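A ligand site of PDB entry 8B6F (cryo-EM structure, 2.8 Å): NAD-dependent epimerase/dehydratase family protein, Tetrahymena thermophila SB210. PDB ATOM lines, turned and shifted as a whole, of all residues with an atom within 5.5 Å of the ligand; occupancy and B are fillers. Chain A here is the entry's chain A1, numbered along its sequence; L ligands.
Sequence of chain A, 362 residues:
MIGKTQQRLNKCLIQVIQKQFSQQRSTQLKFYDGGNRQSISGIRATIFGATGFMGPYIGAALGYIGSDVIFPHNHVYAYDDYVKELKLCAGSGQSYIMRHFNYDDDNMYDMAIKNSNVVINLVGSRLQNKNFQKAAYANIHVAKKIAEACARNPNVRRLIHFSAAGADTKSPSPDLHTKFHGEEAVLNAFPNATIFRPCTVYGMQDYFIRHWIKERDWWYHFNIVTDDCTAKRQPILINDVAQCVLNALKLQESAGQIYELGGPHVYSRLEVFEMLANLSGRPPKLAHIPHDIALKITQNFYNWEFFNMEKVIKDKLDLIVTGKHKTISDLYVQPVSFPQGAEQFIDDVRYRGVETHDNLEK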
ATOM      1  N   GLY A  49      19.264 -21.083  17.869  1.00  0.00           N
ATOM      2  CA  GLY A  49      20.674 -20.731  17.950  1.00  0.00           C
ATOM      3  C   GLY A  49      21.594 -21.898  18.193  1.00  0.00           C
ATOM      4  O   GLY A  49      22.519 -21.801  19.006  1.00  0.00           O
ATOM      5  N   ALA A  50      21.375 -23.018  17.492  1.00  0.00           N
ATOM      6  CA  ALA A  50      22.186 -24.210  17.657  1.00  0.00           C
ATOM      7  C   ALA A  50      23.401 -24.256  16.746  1.00  0.00           C
ATOM      8  O   ALA A  50      24.146 -25.230  16.781  1.00  0.00           O
ATOM      9  CB  ALA A  50      21.322 -25.460  17.419  1.00  0.00           C
ATOM     10  N   THR A  51      23.617 -23.217  15.939  1.00  0.00           N
ATOM     11  CA  THR A  51      24.759 -23.177  15.030  1.00  0.00           C
ATOM     12  C   THR A  51      26.035 -22.699  15.706  1.00  0.00           C
ATOM     13  O   THR A  51      27.076 -22.628  15.040  1.00  0.00           O
ATOM     14  CB  THR A  51      24.457 -22.289  13.832  1.00  0.00           C
ATOM     15  OG1 THR A  51      24.063 -20.981  14.281  1.00  0.00           O
ATOM     16  CG2 THR A  51      23.336 -22.885  12.988  1.00  0.00           C
ATOM     17  N   GLY A  52      25.990 -22.359  16.994  1.00  0.00           N
ATOM     18  CA  GLY A  52      27.157 -21.915  17.716  1.00  0.00           C
ATOM     19  C   GLY A  52      28.009 -23.060  18.208  1.00  0.00           C
ATOM     20  O   GLY A  52      27.818 -24.231  17.856  1.00  0.00           O
ATOM     21  N   PHE A  53      28.982 -22.718  19.046  1.00  0.00           N
ATOM     22  CA  PHE A  53      29.889 -23.723  19.584  1.00  0.00           C
ATOM     23  C   PHE A  53      29.148 -24.737  20.436  1.00  0.00           C
ATOM     24  O   PHE A  53      29.407 -25.950  20.348  1.00  0.00           O
ATOM     25  CB  PHE A  53      31.001 -23.046  20.396  1.00  0.00           C
ATOM     26  CG  PHE A  53      31.503 -23.874  21.545  1.00  0.00           C
ATOM     27  CD1 PHE A  53      32.187 -25.058  21.314  1.00  0.00           C
ATOM     28  CD2 PHE A  53      31.334 -23.451  22.850  1.00  0.00           C
ATOM     29  CE1 PHE A  53      32.654 -25.820  22.366  1.00  0.00           C
ATOM     30  CE2 PHE A  53      31.795 -24.200  23.905  1.00  0.00           C
ATOM     31  CZ  PHE A  53      32.471 -25.394  23.666  1.00  0.00           C
ATOM     32  N   MET A  54      28.237 -24.275  21.280  1.00  0.00           N
ATOM     33  CA  MET A  54      27.549 -25.138  22.236  1.00  0.00           C
ATOM     34  C   MET A  54      26.294 -25.780  21.678  1.00  0.00           C
ATOM     35  O   MET A  54      25.763 -26.708  22.295  1.00  0.00           O
ATOM     36  CB  MET A  54      27.217 -24.327  23.490  1.00  0.00           C
ATOM     37  CG  MET A  54      26.845 -25.163  24.699  1.00  0.00           C
ATOM     38  SD  MET A  54      27.119 -24.277  26.245  1.00  0.00           S
ATOM     39  CE  MET A  54      26.185 -22.779  25.932  1.00  0.00           C
ATOM     40  N   GLY A  55      25.807 -25.315  20.531  1.00  0.00           N
ATOM     41  CA  GLY A  55      24.567 -25.793  19.971  1.00  0.00           C
ATOM     42  C   GLY A  55      24.559 -27.275  19.656  1.00  0.00           C
ATOM     43  O   GLY A  55      23.667 -28.017  20.073  1.00  0.00           O
ATOM     44  N   ASN A  74      19.134 -19.452  10.519  1.00  0.00           N
ATOM     45  CA  ASN A  74      19.358 -18.658   9.310  1.00  0.00           C
ATOM     46  C   ASN A  74      20.851 -18.330   9.337  1.00  0.00           C
ATOM     47  O   ASN A  74      21.255 -17.257   9.784  1.00  0.00           O
ATOM     48  CB  ASN A  74      18.482 -17.412   9.278  1.00  0.00           C
ATOM     49  CG  ASN A  74      18.539 -16.707   7.944  1.00  0.00           C
ATOM     50  OD1 ASN A  74      18.899 -17.293   6.928  1.00  0.00           O
ATOM     51  ND2 ASN A  74      18.175 -15.427   7.939  1.00  0.00           N
ATOM     52  N   HIS A  75      21.676 -19.293   8.913  1.00  0.00           N
ATOM     53  CA  HIS A  75      23.157 -19.195   8.998  1.00  0.00           C
ATOM     54  C   HIS A  75      23.845 -19.070   7.645  1.00  0.00           C
ATOM     55  O   HIS A  75      23.428 -19.779   6.732  1.00  0.00           O
ATOM     56  CB  HIS A  75      23.703 -20.457   9.629  1.00  0.00           C
ATOM     57  CG  HIS A  75      25.167 -20.471   9.884  1.00  0.00           C
ATOM     58  ND1 HIS A  75      25.749 -19.722  10.879  1.00  0.00           N
ATOM     59  CD2 HIS A  75      26.172 -21.176   9.314  1.00  0.00           C
ATOM     60  CE1 HIS A  75      27.041 -19.938  10.902  1.00  0.00           C
ATOM     61  NE2 HIS A  75      27.325 -20.816   9.957  1.00  0.00           N
ATOM     62  N   VAL A  76      24.874 -18.247   7.550  1.00  0.00           N
ATOM     63  CA  VAL A  76      25.703 -18.096   6.337  1.00  0.00           C
ATOM     64  C   VAL A  76      27.097 -18.536   6.753  1.00  0.00           C
ATOM     65  O   VAL A  76      27.534 -18.073   7.798  1.00  0.00           O
ATOM     66  CB  VAL A  76      25.689 -16.647   5.842  1.00  0.00           C
ATOM     67  CG1 VAL A  76      26.610 -16.436   4.647  1.00  0.00           C
ATOM     68  CG2 VAL A  76      24.281 -16.186   5.523  1.00  0.00           C
ATOM     69  N   TYR A 103      13.469 -14.242  12.063  1.00  0.00           N
ATOM     70  CA  TYR A 103      13.487 -13.998  13.500  1.00  0.00           C
ATOM     71  C   TYR A 103      12.564 -12.876  13.937  1.00  0.00           C
ATOM     72  O   TYR A 103      12.476 -12.592  15.135  1.00  0.00           O
ATOM     73  CB  TYR A 103      14.919 -13.681  13.954  1.00  0.00           C
ATOM     74  CG  TYR A 103      15.827 -14.884  13.922  1.00  0.00           C
ATOM     75  CD1 TYR A 103      15.755 -15.871  14.901  1.00  0.00           C
ATOM     76  CD2 TYR A 103      16.770 -15.038  12.907  1.00  0.00           C
ATOM     77  CE1 TYR A 103      16.587 -16.966  14.871  1.00  0.00           C
ATOM     78  CE2 TYR A 103      17.602 -16.133  12.878  1.00  0.00           C
ATOM     79  CZ  TYR A 103      17.503 -17.101  13.859  1.00  0.00           C
ATOM     80  OH  TYR A 103      18.337 -18.187  13.828  1.00  0.00           O
ATOM     81  N   LEU A 122      19.664 -20.548  22.707  1.00  0.00           N
ATOM     82  CA  LEU A 122      21.070 -20.193  22.801  1.00  0.00           C
ATOM     83  C   LEU A 122      21.419 -19.024  21.877  1.00  0.00           C
ATOM     84  O   LEU A 122      22.594 -18.810  21.576  1.00  0.00           O
ATOM     85  CB  LEU A 122      21.965 -21.391  22.483  1.00  0.00           C
ATOM     86  CG  LEU A 122      21.712 -22.708  23.215  1.00  0.00           C
ATOM     87  CD1 LEU A 122      20.577 -23.484  22.575  1.00  0.00           C
ATOM     88  CD2 LEU A 122      22.980 -23.551  23.245  1.00  0.00           C
ATOM     89  N   VAL A 123      20.417 -18.296  21.407  1.00  0.00           N
ATOM     90  CA  VAL A 123      20.621 -17.191  20.481  1.00  0.00           C
ATOM     91  C   VAL A 123      21.165 -16.019  21.293  1.00  0.00           C
ATOM     92  O   VAL A 123      20.417 -15.308  21.965  1.00  0.00           O
ATOM     93  CB  VAL A 123      19.336 -16.810  19.740  1.00  0.00           C
ATOM     94  CG1 VAL A 123      19.551 -15.566  18.894  1.00  0.00           C
ATOM     95  CG2 VAL A 123      18.857 -17.966  18.883  1.00  0.00           C
ATOM     96  N   GLY A 124      22.483 -15.814  21.234  1.00  0.00           N
ATOM     97  CA  GLY A 124      23.108 -14.694  21.892  1.00  0.00           C
ATOM     98  C   GLY A 124      24.038 -13.976  20.938  1.00  0.00           C
ATOM     99  O   GLY A 124      24.481 -14.519  19.935  1.00  0.00           O
ATOM    100  N   SER A 125      24.325 -12.719  21.273  1.00  0.00           N
ATOM    101  CA  SER A 125      25.218 -11.912  20.459  1.00  0.00           C
ATOM    102  C   SER A 125      26.566 -12.617  20.331  1.00  0.00           C
ATOM    103  O   SER A 125      27.131 -13.079  21.325  1.00  0.00           O
ATOM    104  CB  SER A 125      25.384 -10.529  21.066  1.00  0.00           C
ATOM    105  OG  SER A 125      26.261  -9.731  20.296  1.00  0.00           O
ATOM    106  N   ARG A 126      27.066 -12.689  19.105  1.00  0.00           N
ATOM    107  CA  ARG A 126      28.342 -13.339  18.866  1.00  0.00           C
ATOM    108  C   ARG A 126      29.495 -12.459  19.347  1.00  0.00           C
ATOM    109  O   ARG A 126      29.388 -11.240  19.424  1.00  0.00           O
ATOM    110  CB  ARG A 126      28.516 -13.678  17.388  1.00  0.00           C
ATOM    111  CG  ARG A 126      27.842 -14.973  16.974  1.00  0.00           C
ATOM    112  CD  ARG A 126      28.215 -15.360  15.551  1.00  0.00           C
ATOM    113  NE  ARG A 126      27.804 -16.724  15.239  1.00  0.00           N
ATOM    114  CZ  ARG A 126      28.513 -17.812  15.522  1.00  0.00           C
ATOM    115  NH1 ARG A 126      29.680 -17.725  16.142  1.00  0.00           N
ATOM    116  NH2 ARG A 126      28.044 -19.006  15.179  1.00  0.00           N
ATOM    117  N   LEU A 127      30.615 -13.112  19.663  1.00  0.00           N
ATOM    118  CA  LEU A 127      31.806 -12.391  20.084  1.00  0.00           C
ATOM    119  C   LEU A 127      32.340 -11.488  18.981  1.00  0.00           C
ATOM    120  O   LEU A 127      33.150 -10.599  19.245  1.00  0.00           O
ATOM    121  CB  LEU A 127      32.885 -13.369  20.521  1.00  0.00           C
ATOM    122  CG  LEU A 127      34.038 -12.778  21.337  1.00  0.00           C
ATOM    123  CD1 LEU A 127      33.581 -12.423  22.736  1.00  0.00           C
ATOM    124  CD2 LEU A 127      35.204 -13.747  21.378  1.00  0.00           C
ATOM    125  N   LYS A 134      22.695  -4.315  17.249  1.00  0.00           N
ATOM    126  CA  LYS A 134      22.619  -5.718  16.855  1.00  0.00           C
ATOM    127  C   LYS A 134      22.694  -6.631  18.070  1.00  0.00           C
ATOM    128  O   LYS A 134      21.974  -7.631  18.157  1.00  0.00           O
ATOM    129  CB  LYS A 134      23.727  -6.054  15.861  1.00  0.00           C
ATOM    130  CG  LYS A 134      23.509  -5.446  14.480  1.00  0.00           C
ATOM    131  CD  LYS A 134      24.610  -5.869  13.515  1.00  0.00           C
ATOM    132  CE  LYS A 134      24.310  -5.402  12.102  1.00  0.00           C
ATOM    133  NZ  LYS A 134      23.090  -6.066  11.537  1.00  0.00           N
ATOM    134  N   TYR A 137      19.361  -6.511  19.820  1.00  0.00           N
ATOM    135  CA  TYR A 137      18.387  -7.284  19.052  1.00  0.00           C
ATOM    136  C   TYR A 137      18.557  -8.766  19.320  1.00  0.00           C
ATOM    137  O   TYR A 137      17.597  -9.456  19.681  1.00  0.00           O
ATOM    138  CB  TYR A 137      18.561  -6.981  17.555  1.00  0.00           C
ATOM    139  CG  TYR A 137      17.570  -7.707  16.670  1.00  0.00           C
ATOM    140  CD1 TYR A 137      17.858  -8.954  16.150  1.00  0.00           C
ATOM    141  CD2 TYR A 137      16.353  -7.122  16.350  1.00  0.00           C
ATOM    142  CE1 TYR A 137      16.965  -9.611  15.336  1.00  0.00           C
ATOM    143  CE2 TYR A 137      15.443  -7.772  15.544  1.00  0.00           C
ATOM    144  CZ  TYR A 137      15.759  -9.015  15.032  1.00  0.00           C
ATOM    145  OH  TYR A 137      14.850  -9.666  14.226  1.00  0.00           O
ATOM    146  N   ALA A 138      19.770  -9.283  19.134  1.00  0.00           N
ATOM    147  CA  ALA A 138      19.997 -10.721  19.271  1.00  0.00           C
ATOM    148  C   ALA A 138      19.664 -11.203  20.685  1.00  0.00           C
ATOM    149  O   ALA A 138      19.068 -12.267  20.856  1.00  0.00           O
ATOM    150  CB  ALA A 138      21.445 -11.061  18.923  1.00  0.00           C
ATOM    151  N   ASN A 139      20.053 -10.425  21.701  1.00  0.00           N
ATOM    152  CA  ASN A 139      19.947 -10.886  23.077  1.00  0.00           C
ATOM    153  C   ASN A 139      18.599 -10.572  23.734  1.00  0.00           C
ATOM    154  O   ASN A 139      18.327 -11.102  24.814  1.00  0.00           O
ATOM    155  CB  ASN A 139      21.062 -10.278  23.923  1.00  0.00           C
ATOM    156  CG  ASN A 139      22.382 -10.984  23.742  1.00  0.00           C
ATOM    157  OD1 ASN A 139      22.443 -12.217  23.746  1.00  0.00           O
ATOM    158  ND2 ASN A 139      23.456 -10.216  23.592  1.00  0.00           N
ATOM    159  N   VAL A 142      14.926 -11.555  20.056  1.00  0.00           N
ATOM    160  CA  VAL A 142      14.724 -12.968  19.750  1.00  0.00           C
ATOM    161  C   VAL A 142      14.277 -13.725  20.984  1.00  0.00           C
ATOM    162  O   VAL A 142      13.361 -14.555  20.931  1.00  0.00           O
ATOM    163  CB  VAL A 142      16.008 -13.581  19.146  1.00  0.00           C
ATOM    164  CG1 VAL A 142      15.784 -15.040  18.785  1.00  0.00           C
ATOM    165  CG2 VAL A 142      16.451 -12.789  17.924  1.00  0.00           C
ATOM    166  N   PHE A 162      19.566 -19.398  27.685  1.00  0.00           N
ATOM    167  CA  PHE A 162      20.982 -19.350  28.030  1.00  0.00           C
ATOM    168  C   PHE A 162      21.431 -17.900  28.117  1.00  0.00           C
ATOM    169  O   PHE A 162      21.571 -17.228  27.090  1.00  0.00           O
ATOM    170  CB  PHE A 162      21.816 -20.117  27.010  1.00  0.00           C
ATOM    171  CG  PHE A 162      21.986 -21.566  27.346  1.00  0.00           C
ATOM    172  CD1 PHE A 162      20.945 -22.463  27.191  1.00  0.00           C
ATOM    173  CD2 PHE A 162      23.193 -22.037  27.814  1.00  0.00           C
ATOM    174  CE1 PHE A 162      21.098 -23.795  27.498  1.00  0.00           C
ATOM    175  CE2 PHE A 162      23.359 -23.373  28.127  1.00  0.00           C
ATOM    176  CZ  PHE A 162      22.312 -24.256  27.974  1.00  0.00           C
ATOM    177  N   SER A 163      21.649 -17.428  29.332  1.00  0.00           N
ATOM    178  CA  SER A 163      22.234 -16.125  29.589  1.00  0.00           C
ATOM    179  C   SER A 163      23.738 -16.291  29.827  1.00  0.00           C
ATOM    180  O   SER A 163      24.300 -17.379  29.633  1.00  0.00           O
ATOM    181  CB  SER A 163      21.537 -15.454  30.766  1.00  0.00           C
ATOM    182  OG  SER A 163      22.034 -14.153  30.989  1.00  0.00           O
ATOM    183  N   ALA A 164      24.402 -15.224  30.252  1.00  0.00           N
ATOM    184  CA  ALA A 164      25.827 -15.244  30.527  1.00  0.00           C
ATOM    185  C   ALA A 164      26.090 -14.879  31.981  1.00  0.00           C
ATOM    186  O   ALA A 164      25.382 -14.050  32.551  1.00  0.00           O
ATOM    187  CB  ALA A 164      26.576 -14.266  29.604  1.00  0.00           C
ATOM    188  N   ALA A 165      27.106 -15.505  32.565  1.00  0.00           N
ATOM    189  CA  ALA A 165      27.508 -15.177  33.924  1.00  0.00           C
ATOM    190  C   ALA A 165      28.065 -13.757  33.967  1.00  0.00           C
ATOM    191  O   ALA A 165      28.781 -13.326  33.065  1.00  0.00           O
ATOM    192  CB  ALA A 165      28.544 -16.172  34.429  1.00  0.00           C
ATOM    193  N   LYS A 179      22.140  -8.943  27.621  1.00  0.00           N
ATOM    194  CA  LYS A 179      21.704 -10.241  28.098  1.00  0.00           C
ATOM    195  C   LYS A 179      20.918 -10.124  29.404  1.00  0.00           C
ATOM    196  O   LYS A 179      19.997 -10.912  29.634  1.00  0.00           O
ATOM    197  CB  LYS A 179      22.895 -11.181  28.283  1.00  0.00           C
ATOM    198  CG  LYS A 179      23.354 -11.825  26.992  1.00  0.00           C
ATOM    199  CD  LYS A 179      24.529 -12.773  27.221  1.00  0.00           C
ATOM    200  CE  LYS A 179      25.014 -13.344  25.903  1.00  0.00           C
ATOM    201  NZ  LYS A 179      26.343 -14.007  26.032  1.00  0.00           N
ATOM    202  N   PRO A 198      26.176 -19.698  32.376  1.00  0.00           N
ATOM    203  CA  PRO A 198      27.459 -20.412  32.384  1.00  0.00           C
ATOM    204  C   PRO A 198      28.633 -19.449  32.423  1.00  0.00           C
ATOM    205  O   PRO A 198      28.563 -18.323  31.921  1.00  0.00           O
ATOM    206  CB  PRO A 198      27.449 -21.215  31.082  1.00  0.00           C
ATOM    207  CG  PRO A 198      26.033 -21.173  30.599  1.00  0.00           C
ATOM    208  CD  PRO A 198      25.468 -19.889  31.104  1.00  0.00           C
ATOM    209  N   CYS A 199      29.716 -19.910  33.035  1.00  0.00           N
ATOM    210  CA  CYS A 199      30.997 -19.208  32.970  1.00  0.00           C
ATOM    211  C   CYS A 199      31.660 -19.539  31.632  1.00  0.00           C
ATOM    212  O   CYS A 199      31.035 -20.081  30.721  1.00  0.00           O
ATOM    213  CB  CYS A 199      31.835 -19.585  34.180  1.00  0.00           C
ATOM    214  SG  CYS A 199      31.134 -18.974  35.722  1.00  0.00           S
ATOM    215  N   THR A 200      32.939 -19.200  31.488  1.00  0.00           N
ATOM    216  CA  THR A 200      33.627 -19.459  30.237  1.00  0.00           C
ATOM    217  C   THR A 200      33.685 -20.952  29.967  1.00  0.00           C
ATOM    218  O   THR A 200      34.444 -21.673  30.607  1.00  0.00           O
ATOM    219  CB  THR A 200      35.030 -18.862  30.258  1.00  0.00           C
ATOM    220  OG1 THR A 200      34.962 -17.451  30.524  1.00  0.00           O
ATOM    221  CG2 THR A 200      35.730 -19.066  28.919  1.00  0.00           C
ATOM    222  N   VAL A 201      32.895 -21.423  29.004  1.00  0.00           N
ATOM    223  CA  VAL A 201      32.856 -22.837  28.669  1.00  0.00           C
ATOM    224  C   VAL A 201      34.002 -23.156  27.711  1.00  0.00           C
ATOM    225  O   VAL A 201      34.265 -22.408  26.776  1.00  0.00           O
ATOM    226  CB  VAL A 201      31.495 -23.206  28.045  1.00  0.00           C
ATOM    227  CG1 VAL A 201      31.400 -24.712  27.810  1.00  0.00           C
ATOM    228  CG2 VAL A 201      30.358 -22.734  28.927  1.00  0.00           C
ATOM    229  N   TYR A 207      35.728 -21.136  22.318  1.00  0.00           N
ATOM    230  CA  TYR A 207      36.361 -19.854  22.009  1.00  0.00           C
ATOM    231  C   TYR A 207      37.452 -19.499  22.999  1.00  0.00           C
ATOM    232  O   TYR A 207      37.945 -18.368  22.971  1.00  0.00           O
ATOM    233  CB  TYR A 207      35.314 -18.748  21.980  1.00  0.00           C
ATOM    234  CG  TYR A 207      34.228 -18.943  20.949  1.00  0.00           C
ATOM    235  CD1 TYR A 207      34.448 -18.668  19.610  1.00  0.00           C
ATOM    236  CD2 TYR A 207      32.959 -19.380  21.328  1.00  0.00           C
ATOM    237  CE1 TYR A 207      33.459 -18.832  18.674  1.00  0.00           C
ATOM    238  CE2 TYR A 207      31.967 -19.554  20.394  1.00  0.00           C
ATOM    239  CZ  TYR A 207      32.217 -19.284  19.072  1.00  0.00           C
ATOM    240  OH  TYR A 207      31.225 -19.458  18.139  1.00  0.00           O
HETATM  241  P1  LIG L   1      27.625 -18.511  19.812  1.00  0.00           P
HETATM  242  O1  LIG L   1      28.084 -17.068  19.646  1.00  0.00           O
HETATM  243  O2  LIG L   1      28.572 -19.542  19.214  1.00  0.00           O
HETATM  244  O3  LIG L   1      26.133 -18.770  19.174  1.00  0.00           O
HETATM  245  C1  LIG L   1      25.166 -17.743  19.129  1.00  0.00           C
HETATM  246  C2  LIG L   1      23.970 -18.244  18.276  1.00  0.00           C
HETATM  247  O4  LIG L   1      23.089 -17.292  18.132  1.00  0.00           O
HETATM  248  C3  LIG L   1      24.454 -18.599  16.862  1.00  0.00           C
HETATM  249  O5  LIG L   1      23.780 -19.689  16.409  1.00  0.00           O
HETATM  250  C4  LIG L   1      24.093 -17.367  16.012  1.00  0.00           C
HETATM  251  O6  LIG L   1      23.845 -17.791  14.608  1.00  0.00           O
HETATM  252  C5  LIG L   1      23.006 -16.916  16.564  1.00  0.00           C
HETATM  253  N1  LIG L   1      22.871 -15.481  16.447  1.00  0.00           N
HETATM  254  C6  LIG L   1      23.778 -14.558  16.762  1.00  0.00           C
HETATM  255  N2  LIG L   1      23.250 -13.358  16.517  1.00  0.00           N
HETATM  256  C7  LIG L   1      22.012 -13.555  16.050  1.00  0.00           C
HETATM  257  C8  LIG L   1      21.052 -12.680  15.645  1.00  0.00           C
HETATM  258  N3  LIG L   1      21.033 -11.258  15.580  1.00  0.00           N
HETATM  259  N4  LIG L   1      19.876 -13.122  15.208  1.00  0.00           N
HETATM  260  C9  LIG L   1      19.645 -14.446  15.174  1.00  0.00           C
HETATM  261  N5  LIG L   1      20.590 -15.309  15.564  1.00  0.00           N
HETATM  262  C10 LIG L   1      21.773 -14.857  16.008  1.00  0.00           C
HETATM  263  O7  LIG L   1      27.411 -18.913  21.400  1.00  0.00           O
HETATM  264  P2  LIG L   1      27.934 -20.333  22.059  1.00  0.00           P
HETATM  265  O8  LIG L   1      27.724 -21.501  21.107  1.00  0.00           O
HETATM  266  O9  LIG L   1      29.355 -20.120  22.498  1.00  0.00           O
HETATM  267  O10 LIG L   1      27.053 -20.542  23.446  1.00  0.00           O
HETATM  268  C11 LIG L   1      25.622 -20.451  23.386  1.00  0.00           C
HETATM  269  C12 LIG L   1      25.128 -19.307  24.231  1.00  0.00           C
HETATM  270  O11 LIG L   1      25.486 -19.539  25.460  1.00  0.00           O
HETATM  271  C13 LIG L   1      25.811 -17.844  23.835  1.00  0.00           C
HETATM  272  O12 LIG L   1      25.029 -17.173  22.768  1.00  0.00           O
HETATM  273  C14 LIG L   1      25.765 -17.169  24.865  1.00  0.00           C
HETATM  274  O13 LIG L   1      24.475 -16.381  24.904  1.00  0.00           O
HETATM  275  C15 LIG L   1      25.780 -18.212  26.082  1.00  0.00           C
HETATM  276  N6  LIG L   1      26.987 -18.227  26.673  1.00  0.00           N
HETATM  277  C16 LIG L   1      28.133 -18.805  25.981  1.00  0.00           C
HETATM  278  C17 LIG L   1      29.515 -18.827  26.639  1.00  0.00           C
HETATM  279  C18 LIG L   1      30.689 -19.470  25.867  1.00  0.00           C
HETATM  280  O14 LIG L   1      30.477 -20.240  25.007  1.00  0.00           O
HETATM  281  N7  LIG L   1      32.079 -19.127  26.218  1.00  0.00           N
HETATM  282  C19 LIG L   1      29.766 -18.249  28.025  1.00  0.00           C
HETATM  283  C20 LIG L   1      28.529 -17.665  28.719  1.00  0.00           C
HETATM  284  C21 LIG L   1      27.155 -17.650  28.034  1.00  0.00           C
HETATM  285  P3  LIG L   1      24.797 -17.222  13.388  1.00  0.00           P
HETATM  286  O15 LIG L   1      25.418 -15.901  13.750  1.00  0.00           O
HETATM  287  O16 LIG L   1      25.872 -18.249  13.085  1.00  0.00           O
HETATM  288  O17 LIG L   1      23.962 -17.110  12.128  1.00  0.00           O
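The side-chain hydroxyl of Tyr 207 lies within hydrogen-bond range of the guanidinium group of Arg 126, 3.1 Å away. The backbone carbonyl oxygen of Pro 198 sits at hydrogen-bond distance from the backbone NH of Ala 165. The backbone carbonyl oxygen of Tyr 137 sits at hydrogen-bond distance from the backbone NH of Val 142 (3.4 Å).
Gly 49 touches the ligand. Gly 52 touches the ligand (CA to O2, 3.1 Å). Asn 74 touches the ligand (O to O17, 3.6 Å). Tyr 103 touches the ligand (CE2 to C9, 3.5 Å). Val 123 touches the ligand (CA to O4, 3.4 Å). CD1 of Tyr 137 touches N3 of the ligand, at 3.96 Å. CB of Ala 138 touches N3 of the ligand, 3.4 Å away. Phe 162 touches the ligand. O of Ser 163 touches C21 of the ligand, 3.3 Å away. Ala 164 touches the ligand. Pro 198 touches the ligand. O of Cys 199 touches C19 of the ligand (3.5 Å). Val 201 touches the ligand. Hydrophobic or aromatic side chains within 4 Å of the ligand: Phe 53, Met 54, His 75, Tyr 103, Leu 122, Val 123, Tyr 137, Ala 138, Ala 164 and Tyr 207. Within 4 Å of the ligand: Gly 49, Thr 51, Gly 52, Phe 53, Met 54, Asn 74, His 75, Tyr 103, Leu 122, Val 123, Gly 124, Arg 126, Tyr 137, Ala 138, Phe 162, Ser 163, Ala 164, Lys 179, Pro 198, Cys 199, Val 201 and Tyr 207.
OG1 of Thr 51 is in hydrogen-bond range of O5 of the ligand, 2.5 Å away. ND1 of His 75 lies within hydrogen-bond range of O16 of the ligand. The backbone NH (N) of Phe 53 lies within hydrogen-bond range of an oxygen (O8) of the ligand, at 2.7 Å. The backbone NH (N) of Met 54 is in hydrogen-bond range of an oxygen (O8) of the ligand (2.8 Å). OH of Tyr 207 is in hydrogen-bond range of O2 of the ligand, 2.9 Å away. NE of Arg 126 is in salt-bridge range of O15 of the ligand (2.9 Å). O12 of the ligand sits at hydrogen-bond distance from O of Leu 122. NZ of Lys 179 lies within hydrogen-bond range of O13 of the ligand, 3.2 Å away. An oxygen (O12) of the ligand sits close to the backbone NH of Gly 124.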
